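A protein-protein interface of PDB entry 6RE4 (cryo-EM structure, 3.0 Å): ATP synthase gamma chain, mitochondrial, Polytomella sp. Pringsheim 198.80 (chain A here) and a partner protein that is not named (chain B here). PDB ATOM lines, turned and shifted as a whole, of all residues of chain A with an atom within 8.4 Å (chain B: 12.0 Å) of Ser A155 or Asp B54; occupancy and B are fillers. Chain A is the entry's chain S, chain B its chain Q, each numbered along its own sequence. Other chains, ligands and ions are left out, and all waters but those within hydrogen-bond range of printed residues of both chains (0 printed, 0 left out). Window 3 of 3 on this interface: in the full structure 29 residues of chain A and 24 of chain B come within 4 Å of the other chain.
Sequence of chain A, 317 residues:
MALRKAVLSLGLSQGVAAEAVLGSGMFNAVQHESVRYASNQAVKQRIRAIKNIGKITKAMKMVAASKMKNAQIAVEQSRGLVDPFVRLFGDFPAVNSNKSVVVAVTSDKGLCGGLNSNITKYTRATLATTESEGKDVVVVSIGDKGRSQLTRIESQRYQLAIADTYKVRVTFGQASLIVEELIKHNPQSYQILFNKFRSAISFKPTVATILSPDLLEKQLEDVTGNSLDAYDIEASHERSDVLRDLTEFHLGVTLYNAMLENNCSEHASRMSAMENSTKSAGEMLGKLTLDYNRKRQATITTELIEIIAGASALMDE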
ATOM      1  N   VAL A 139      -7.491  15.940  -8.795  1.00  0.00           N
ATOM      2  CA  VAL A 139      -8.810  15.351  -8.959  1.00  0.00           C
ATOM      3  C   VAL A 139      -8.934  14.197  -7.980  1.00  0.00           C
ATOM      4  O   VAL A 139      -8.081  13.304  -7.951  1.00  0.00           O
ATOM      5  CB  VAL A 139      -9.046  14.890 -10.401  1.00  0.00           C
ATOM      6  CG1 VAL A 139     -10.444  14.363 -10.552  1.00  0.00           C
ATOM      7  CG2 VAL A 139      -8.800  16.030 -11.355  1.00  0.00           C
ATOM      8  N   LEU A 150     -13.057   8.601 -14.259  1.00  0.00           N
ATOM      9  CA  LEU A 150     -12.275   9.826 -14.275  1.00  0.00           C
ATOM     10  C   LEU A 150     -10.900   9.617 -14.875  1.00  0.00           C
ATOM     11  O   LEU A 150     -10.418  10.491 -15.599  1.00  0.00           O
ATOM     12  CB  LEU A 150     -12.149  10.392 -12.863  1.00  0.00           C
ATOM     13  CG  LEU A 150     -13.348  11.249 -12.457  1.00  0.00           C
ATOM     14  CD1 LEU A 150     -13.186  11.775 -11.055  1.00  0.00           C
ATOM     15  CD2 LEU A 150     -13.522  12.371 -13.441  1.00  0.00           C
ATOM     16  N   THR A 151     -10.276   8.466 -14.623  1.00  0.00           N
ATOM     17  CA  THR A 151      -9.001   8.151 -15.251  1.00  0.00           C
ATOM     18  C   THR A 151      -9.119   7.907 -16.748  1.00  0.00           C
ATOM     19  O   THR A 151      -8.101   7.948 -17.444  1.00  0.00           O
ATOM     20  CB  THR A 151      -8.367   6.938 -14.578  1.00  0.00           C
ATOM     21  OG1 THR A 151      -9.086   5.757 -14.949  1.00  0.00           O
ATOM     22  CG2 THR A 151      -8.369   7.100 -13.071  1.00  0.00           C
ATOM     23  N   ARG A 152     -10.322   7.662 -17.262  1.00  0.00           N
ATOM     24  CA  ARG A 152     -10.484   7.563 -18.703  1.00  0.00           C
ATOM     25  C   ARG A 152     -10.447   8.933 -19.362  1.00  0.00           C
ATOM     26  O   ARG A 152      -9.949   9.060 -20.485  1.00  0.00           O
ATOM     27  CB  ARG A 152     -11.789   6.837 -19.047  1.00  0.00           C
ATOM     28  CG  ARG A 152     -11.893   5.453 -18.422  1.00  0.00           C
ATOM     29  CD  ARG A 152     -12.727   4.489 -19.256  1.00  0.00           C
ATOM     30  NE  ARG A 152     -14.126   4.892 -19.369  1.00  0.00           N
ATOM     31  CZ  ARG A 152     -15.102   4.486 -18.560  1.00  0.00           C
ATOM     32  NH1 ARG A 152     -16.342   4.906 -18.756  1.00  0.00           N
ATOM     33  NH2 ARG A 152     -14.843   3.670 -17.548  1.00  0.00           N
ATOM     34  N   ILE A 153     -10.943   9.963 -18.685  1.00  0.00           N
ATOM     35  CA  ILE A 153     -10.949  11.289 -19.284  1.00  0.00           C
ATOM     36  C   ILE A 153      -9.701  12.084 -18.905  1.00  0.00           C
ATOM     37  O   ILE A 153      -9.338  13.033 -19.608  1.00  0.00           O
ATOM     38  CB  ILE A 153     -12.243  12.042 -18.907  1.00  0.00           C
ATOM     39  CG1 ILE A 153     -12.563  13.140 -19.928  1.00  0.00           C
ATOM     40  CG2 ILE A 153     -12.183  12.609 -17.498  1.00  0.00           C
ATOM     41  CD1 ILE A 153     -12.798  12.623 -21.332  1.00  0.00           C
ATOM     42  N   GLU A 154      -9.001  11.674 -17.846  1.00  0.00           N
ATOM     43  CA  GLU A 154      -7.887  12.449 -17.297  1.00  0.00           C
ATOM     44  C   GLU A 154      -7.123  11.558 -16.324  1.00  0.00           C
ATOM     45  O   GLU A 154      -7.680  11.141 -15.307  1.00  0.00           O
ATOM     46  CB  GLU A 154      -8.433  13.711 -16.631  1.00  0.00           C
ATOM     47  CG  GLU A 154      -7.547  14.411 -15.672  1.00  0.00           C
ATOM     48  CD  GLU A 154      -7.908  14.005 -14.277  1.00  0.00           C
ATOM     49  OE1 GLU A 154      -9.117  13.985 -13.963  1.00  0.00           O
ATOM     50  OE2 GLU A 154      -6.997  13.634 -13.527  1.00  0.00           O
ATOM     51  N   SER A 155      -5.857  11.272 -16.609  1.00  0.00           N
ATOM     52  CA  SER A 155      -5.145  10.286 -15.801  1.00  0.00           C
ATOM     53  C   SER A 155      -4.114  10.890 -14.864  1.00  0.00           C
ATOM     54  O   SER A 155      -3.818  10.302 -13.820  1.00  0.00           O
ATOM     55  CB  SER A 155      -4.453   9.259 -16.699  1.00  0.00           C
ATOM     56  OG  SER A 155      -3.873   8.230 -15.914  1.00  0.00           O
ATOM     57  N   GLN A 156      -3.554  12.045 -15.209  1.00  0.00           N
ATOM     58  CA  GLN A 156      -2.406  12.570 -14.484  1.00  0.00           C
ATOM     59  C   GLN A 156      -2.793  13.419 -13.280  1.00  0.00           C
ATOM     60  O   GLN A 156      -2.108  13.365 -12.254  1.00  0.00           O
ATOM     61  CB  GLN A 156      -1.506  13.370 -15.437  1.00  0.00           C
ATOM     62  CG  GLN A 156      -2.124  14.612 -16.089  1.00  0.00           C
ATOM     63  CD  GLN A 156      -2.951  14.294 -17.320  1.00  0.00           C
ATOM     64  OE1 GLN A 156      -2.725  13.285 -17.987  1.00  0.00           O
ATOM     65  NE2 GLN A 156      -3.924  15.149 -17.620  1.00  0.00           N
ATOM     66  N   ARG A 157      -3.881  14.181 -13.365  1.00  0.00           N
ATOM     67  CA  ARG A 157      -4.293  15.030 -12.259  1.00  0.00           C
ATOM     68  C   ARG A 157      -5.080  14.269 -11.207  1.00  0.00           C
ATOM     69  O   ARG A 157      -5.198  14.746 -10.076  1.00  0.00           O
ATOM     70  CB  ARG A 157      -5.117  16.196 -12.798  1.00  0.00           C
ATOM     71  CG  ARG A 157      -4.483  16.856 -14.002  1.00  0.00           C
ATOM     72  CD  ARG A 157      -4.903  18.295 -14.129  1.00  0.00           C
ATOM     73  NE  ARG A 157      -6.218  18.424 -14.740  1.00  0.00           N
ATOM     74  CZ  ARG A 157      -6.415  18.831 -15.986  1.00  0.00           C
ATOM     75  NH1 ARG A 157      -7.646  18.920 -16.474  1.00  0.00           N
ATOM     76  NH2 ARG A 157      -5.380  19.154 -16.743  1.00  0.00           N
ATOM     77  N   TYR A 158      -5.609  13.104 -11.555  1.00  0.00           N
ATOM     78  CA  TYR A 158      -6.331  12.272 -10.608  1.00  0.00           C
ATOM     79  C   TYR A 158      -5.364  11.683  -9.598  1.00  0.00           C
ATOM     80  O   TYR A 158      -4.443  10.952  -9.968  1.00  0.00           O
ATOM     81  CB  TYR A 158      -7.066  11.167 -11.349  1.00  0.00           C
ATOM     82  CG  TYR A 158      -8.013  10.411 -10.479  1.00  0.00           C
ATOM     83  CD1 TYR A 158      -7.641   9.207  -9.896  1.00  0.00           C
ATOM     84  CD2 TYR A 158      -9.279  10.897 -10.231  1.00  0.00           C
ATOM     85  CE1 TYR A 158      -8.507   8.518  -9.096  1.00  0.00           C
ATOM     86  CE2 TYR A 158     -10.146  10.215  -9.438  1.00  0.00           C
ATOM     87  CZ  TYR A 158      -9.754   9.031  -8.874  1.00  0.00           C
ATOM     88  OH  TYR A 158     -10.629   8.354  -8.080  1.00  0.00           O
ATOM     89  N   GLN A 159      -5.573  11.987  -8.321  1.00  0.00           N
ATOM     90  CA  GLN A 159      -4.604  11.614  -7.313  1.00  0.00           C
ATOM     91  C   GLN A 159      -5.153  10.841  -6.122  1.00  0.00           C
ATOM     92  O   GLN A 159      -4.352  10.365  -5.314  1.00  0.00           O
ATOM     93  CB  GLN A 159      -3.871  12.862  -6.800  1.00  0.00           C
ATOM     94  CG  GLN A 159      -2.988  13.514  -7.847  1.00  0.00           C
ATOM     95  CD  GLN A 159      -2.202  14.678  -7.307  1.00  0.00           C
ATOM     96  OE1 GLN A 159      -2.372  15.068  -6.157  1.00  0.00           O
ATOM     97  NE2 GLN A 159      -1.329  15.236  -8.131  1.00  0.00           N
ATOM     98  N   LEU A 160      -6.467  10.679  -5.988  1.00  0.00           N
ATOM     99  CA  LEU A 160      -7.022  10.070  -4.788  1.00  0.00           C
ATOM    100  C   LEU A 160      -8.390   9.488  -5.101  1.00  0.00           C
ATOM    101  O   LEU A 160      -9.152  10.067  -5.873  1.00  0.00           O
ATOM    102  CB  LEU A 160      -7.119  11.099  -3.658  1.00  0.00           C
ATOM    103  CG  LEU A 160      -7.824  10.780  -2.346  1.00  0.00           C
ATOM    104  CD1 LEU A 160      -7.199   9.582  -1.662  1.00  0.00           C
ATOM    105  CD2 LEU A 160      -7.790  11.993  -1.450  1.00  0.00           C
ATOM    106  N   ALA B  50      -7.257   5.869  -1.444  1.00  0.00           N
ATOM    107  CA  ALA B  50      -6.080   5.360  -2.130  1.00  0.00           C
ATOM    108  C   ALA B  50      -5.413   6.456  -2.948  1.00  0.00           C
ATOM    109  O   ALA B  50      -6.028   7.002  -3.866  1.00  0.00           O
ATOM    110  CB  ALA B  50      -6.455   4.187  -3.029  1.00  0.00           C
ATOM    111  N   PRO B  51      -4.170   6.816  -2.636  1.00  0.00           N
ATOM    112  CA  PRO B  51      -3.466   7.815  -3.447  1.00  0.00           C
ATOM    113  C   PRO B  51      -3.067   7.250  -4.800  1.00  0.00           C
ATOM    114  O   PRO B  51      -2.359   6.246  -4.883  1.00  0.00           O
ATOM    115  CB  PRO B  51      -2.236   8.151  -2.599  1.00  0.00           C
ATOM    116  CG  PRO B  51      -2.598   7.732  -1.218  1.00  0.00           C
ATOM    117  CD  PRO B  51      -3.462   6.539  -1.380  1.00  0.00           C
ATOM    118  N   TYR B  52      -3.498   7.926  -5.860  1.00  0.00           N
ATOM    119  CA  TYR B  52      -3.315   7.482  -7.240  1.00  0.00           C
ATOM    120  C   TYR B  52      -2.187   8.309  -7.851  1.00  0.00           C
ATOM    121  O   TYR B  52      -2.374   9.467  -8.213  1.00  0.00           O
ATOM    122  CB  TYR B  52      -4.611   7.631  -8.023  1.00  0.00           C
ATOM    123  CG  TYR B  52      -5.497   6.411  -7.988  1.00  0.00           C
ATOM    124  CD1 TYR B  52      -6.015   5.878  -9.157  1.00  0.00           C
ATOM    125  CD2 TYR B  52      -5.808   5.785  -6.791  1.00  0.00           C
ATOM    126  CE1 TYR B  52      -6.817   4.760  -9.136  1.00  0.00           C
ATOM    127  CE2 TYR B  52      -6.607   4.666  -6.761  1.00  0.00           C
ATOM    128  CZ  TYR B  52      -7.112   4.160  -7.936  1.00  0.00           C
ATOM    129  OH  TYR B  52      -7.915   3.045  -7.920  1.00  0.00           O
ATOM    130  N   VAL B  53      -1.008   7.701  -7.979  1.00  0.00           N
ATOM    131  CA  VAL B  53       0.180   8.486  -8.302  1.00  0.00           C
ATOM    132  C   VAL B  53       0.222   8.883  -9.773  1.00  0.00           C
ATOM    133  O   VAL B  53       0.760   9.941 -10.121  1.00  0.00           O
ATOM    134  CB  VAL B  53       1.443   7.716  -7.878  1.00  0.00           C
ATOM    135  CG1 VAL B  53       1.581   7.745  -6.374  1.00  0.00           C
ATOM    136  CG2 VAL B  53       1.373   6.280  -8.359  1.00  0.00           C
ATOM    137  N   ASP B  54      -0.332   8.066 -10.657  1.00  0.00           N
ATOM    138  CA  ASP B  54      -0.348   8.387 -12.075  1.00  0.00           C
ATOM    139  C   ASP B  54      -1.682   8.034 -12.714  1.00  0.00           C
ATOM    140  O   ASP B  54      -1.830   8.167 -13.932  1.00  0.00           O
ATOM    141  CB  ASP B  54       0.807   7.668 -12.793  1.00  0.00           C
ATOM    142  CG  ASP B  54       1.159   8.292 -14.135  1.00  0.00           C
ATOM    143  OD1 ASP B  54       1.788   9.368 -14.155  1.00  0.00           O
ATOM    144  OD2 ASP B  54       0.794   7.705 -15.172  1.00  0.00           O
ATOM    145  N   GLY B  55      -2.660   7.609 -11.927  1.00  0.00           N
ATOM    146  CA  GLY B  55      -3.834   6.957 -12.446  1.00  0.00           C
ATOM    147  C   GLY B  55      -3.730   5.460 -12.404  1.00  0.00           C
ATOM    148  O   GLY B  55      -4.471   4.783 -13.122  1.00  0.00           O
ATOM    149  N   LYS B  56      -2.840   4.919 -11.582  1.00  0.00           N
ATOM    150  CA  LYS B  56      -2.492   3.513 -11.664  1.00  0.00           C
ATOM    151  C   LYS B  56      -2.998   2.711 -10.481  1.00  0.00           C
ATOM    152  O   LYS B  56      -3.847   1.829 -10.660  1.00  0.00           O
ATOM    153  CB  LYS B  56      -0.964   3.376 -11.743  1.00  0.00           C
ATOM    154  CG  LYS B  56      -0.317   4.029 -12.949  1.00  0.00           C
ATOM    155  CD  LYS B  56       1.171   3.739 -12.961  1.00  0.00           C
ATOM    156  CE  LYS B  56       1.852   4.400 -14.137  1.00  0.00           C
ATOM    157  NZ  LYS B  56       1.387   3.845 -15.435  1.00  0.00           N
ATOM    158  N   ALA B  57      -2.534   3.027  -9.275  1.00  0.00           N
ATOM    159  CA  ALA B  57      -2.822   2.235  -8.086  1.00  0.00           C
ATOM    160  C   ALA B  57      -2.431   3.045  -6.861  1.00  0.00           C
ATOM    161  O   ALA B  57      -2.130   4.236  -6.952  1.00  0.00           O
ATOM    162  CB  ALA B  57      -2.078   0.892  -8.114  1.00  0.00           C
ATOM    163  N   GLY B  58      -2.409   2.377  -5.718  1.00  0.00           N
ATOM    164  CA  GLY B  58      -1.894   2.955  -4.494  1.00  0.00           C
ATOM    165  C   GLY B  58      -2.337   2.147  -3.299  1.00  0.00           C
ATOM    166  O   GLY B  58      -3.214   1.289  -3.386  1.00  0.00           O
ATOM    167  N   ALA B  59      -1.707   2.439  -2.167  1.00  0.00           N
ATOM    168  CA  ALA B  59      -2.067   1.771  -0.929  1.00  0.00           C
ATOM    169  C   ALA B  59      -3.430   2.257  -0.453  1.00  0.00           C
ATOM    170  O   ALA B  59      -3.870   3.359  -0.769  1.00  0.00           O
ATOM    171  CB  ALA B  59      -1.010   2.022   0.143  1.00  0.00           C
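Hydrophobic or aromatic side chains of chain A that line the printed part of chain B: Tyr A158 and Leu A160. Along chain A the printed residues that touch a printed residue of chain B span positions 155 to 160. Hydrophobic or aromatic side chains of chain B that line the printed part of chain A: Tyr B52. Among the printed residues, no Asp or Glu carboxylate lies within 4 Å of a Lys or Arg side-chain nitrogen of the other chain.
The backbone NH of Tyr B52 is in hydrogen-bond range of the backbone carbonyl oxygen of Gln A159, 2.6 Å away. The side-chain hydroxyl of Ser A155 lies within hydrogen-bond range of the backbone carbonyl oxygen of Asp B54, 2.8 Å away. O of Ser A155 is in hydrogen-bond range of N of Gly B55 (3.5 Å). O of Tyr B52 lies close to O of Tyr A158 (3.1 Å).
Among the printed residues, merely in contact across the chains: Gln A159 with Pro B51 (3.3 Å) and Leu A160 with Ala B50 (3.4 Å).
Val A139 touches none of the printed residues of chain B. No residue of chain B comes within 4 Å of Thr A151. Arg A152 touches none of the printed residues of chain B. No residue of chain B comes within 4 Å of Glu A154. Of chain B, only Asp B54 and Gly B55 come within 4 Å of Ser A155. No residue of chain B comes within 4 Å of Gln A156. No residue of chain B comes within 4 Å of Arg A157. Printed residues of chain B within 4 Å of Tyr A158: Tyr B52. Printed residues of chain B within 4 Å of Gln A159: Pro B51 and Tyr B52. Of the printed residues of chain A, Ala B50 touches Leu A160 (3.4 Å). Asp B54 touches just one residue of chain A: Ser A155 (2.8 Å). Gly B55 touches just one residue of chain A: Ser A155. The nearest residue of chain A that does not touch Asp B54 is Gln A156 (4.4 Å). The nearest printed residue of chain A that does not touch Tyr B52 is Leu A160 (4.1 Å).
The side-chain carboxylate (OD2) of Asp B54 lies within salt-bridge range of the side-chain amino group (NZ) of Lys B56, at 3.9 Å. O of Val A139 lies within hydrogen-bond range of N of Gln A159, 2.9 Å away. The side-chain carboxylate of Glu A154 is in hydrogen-bond range of the backbone NH of Tyr A158, 2.5 Å away. OH of Tyr A158 is in hydrogen-bond range of O of Leu A160 (3.2 Å).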
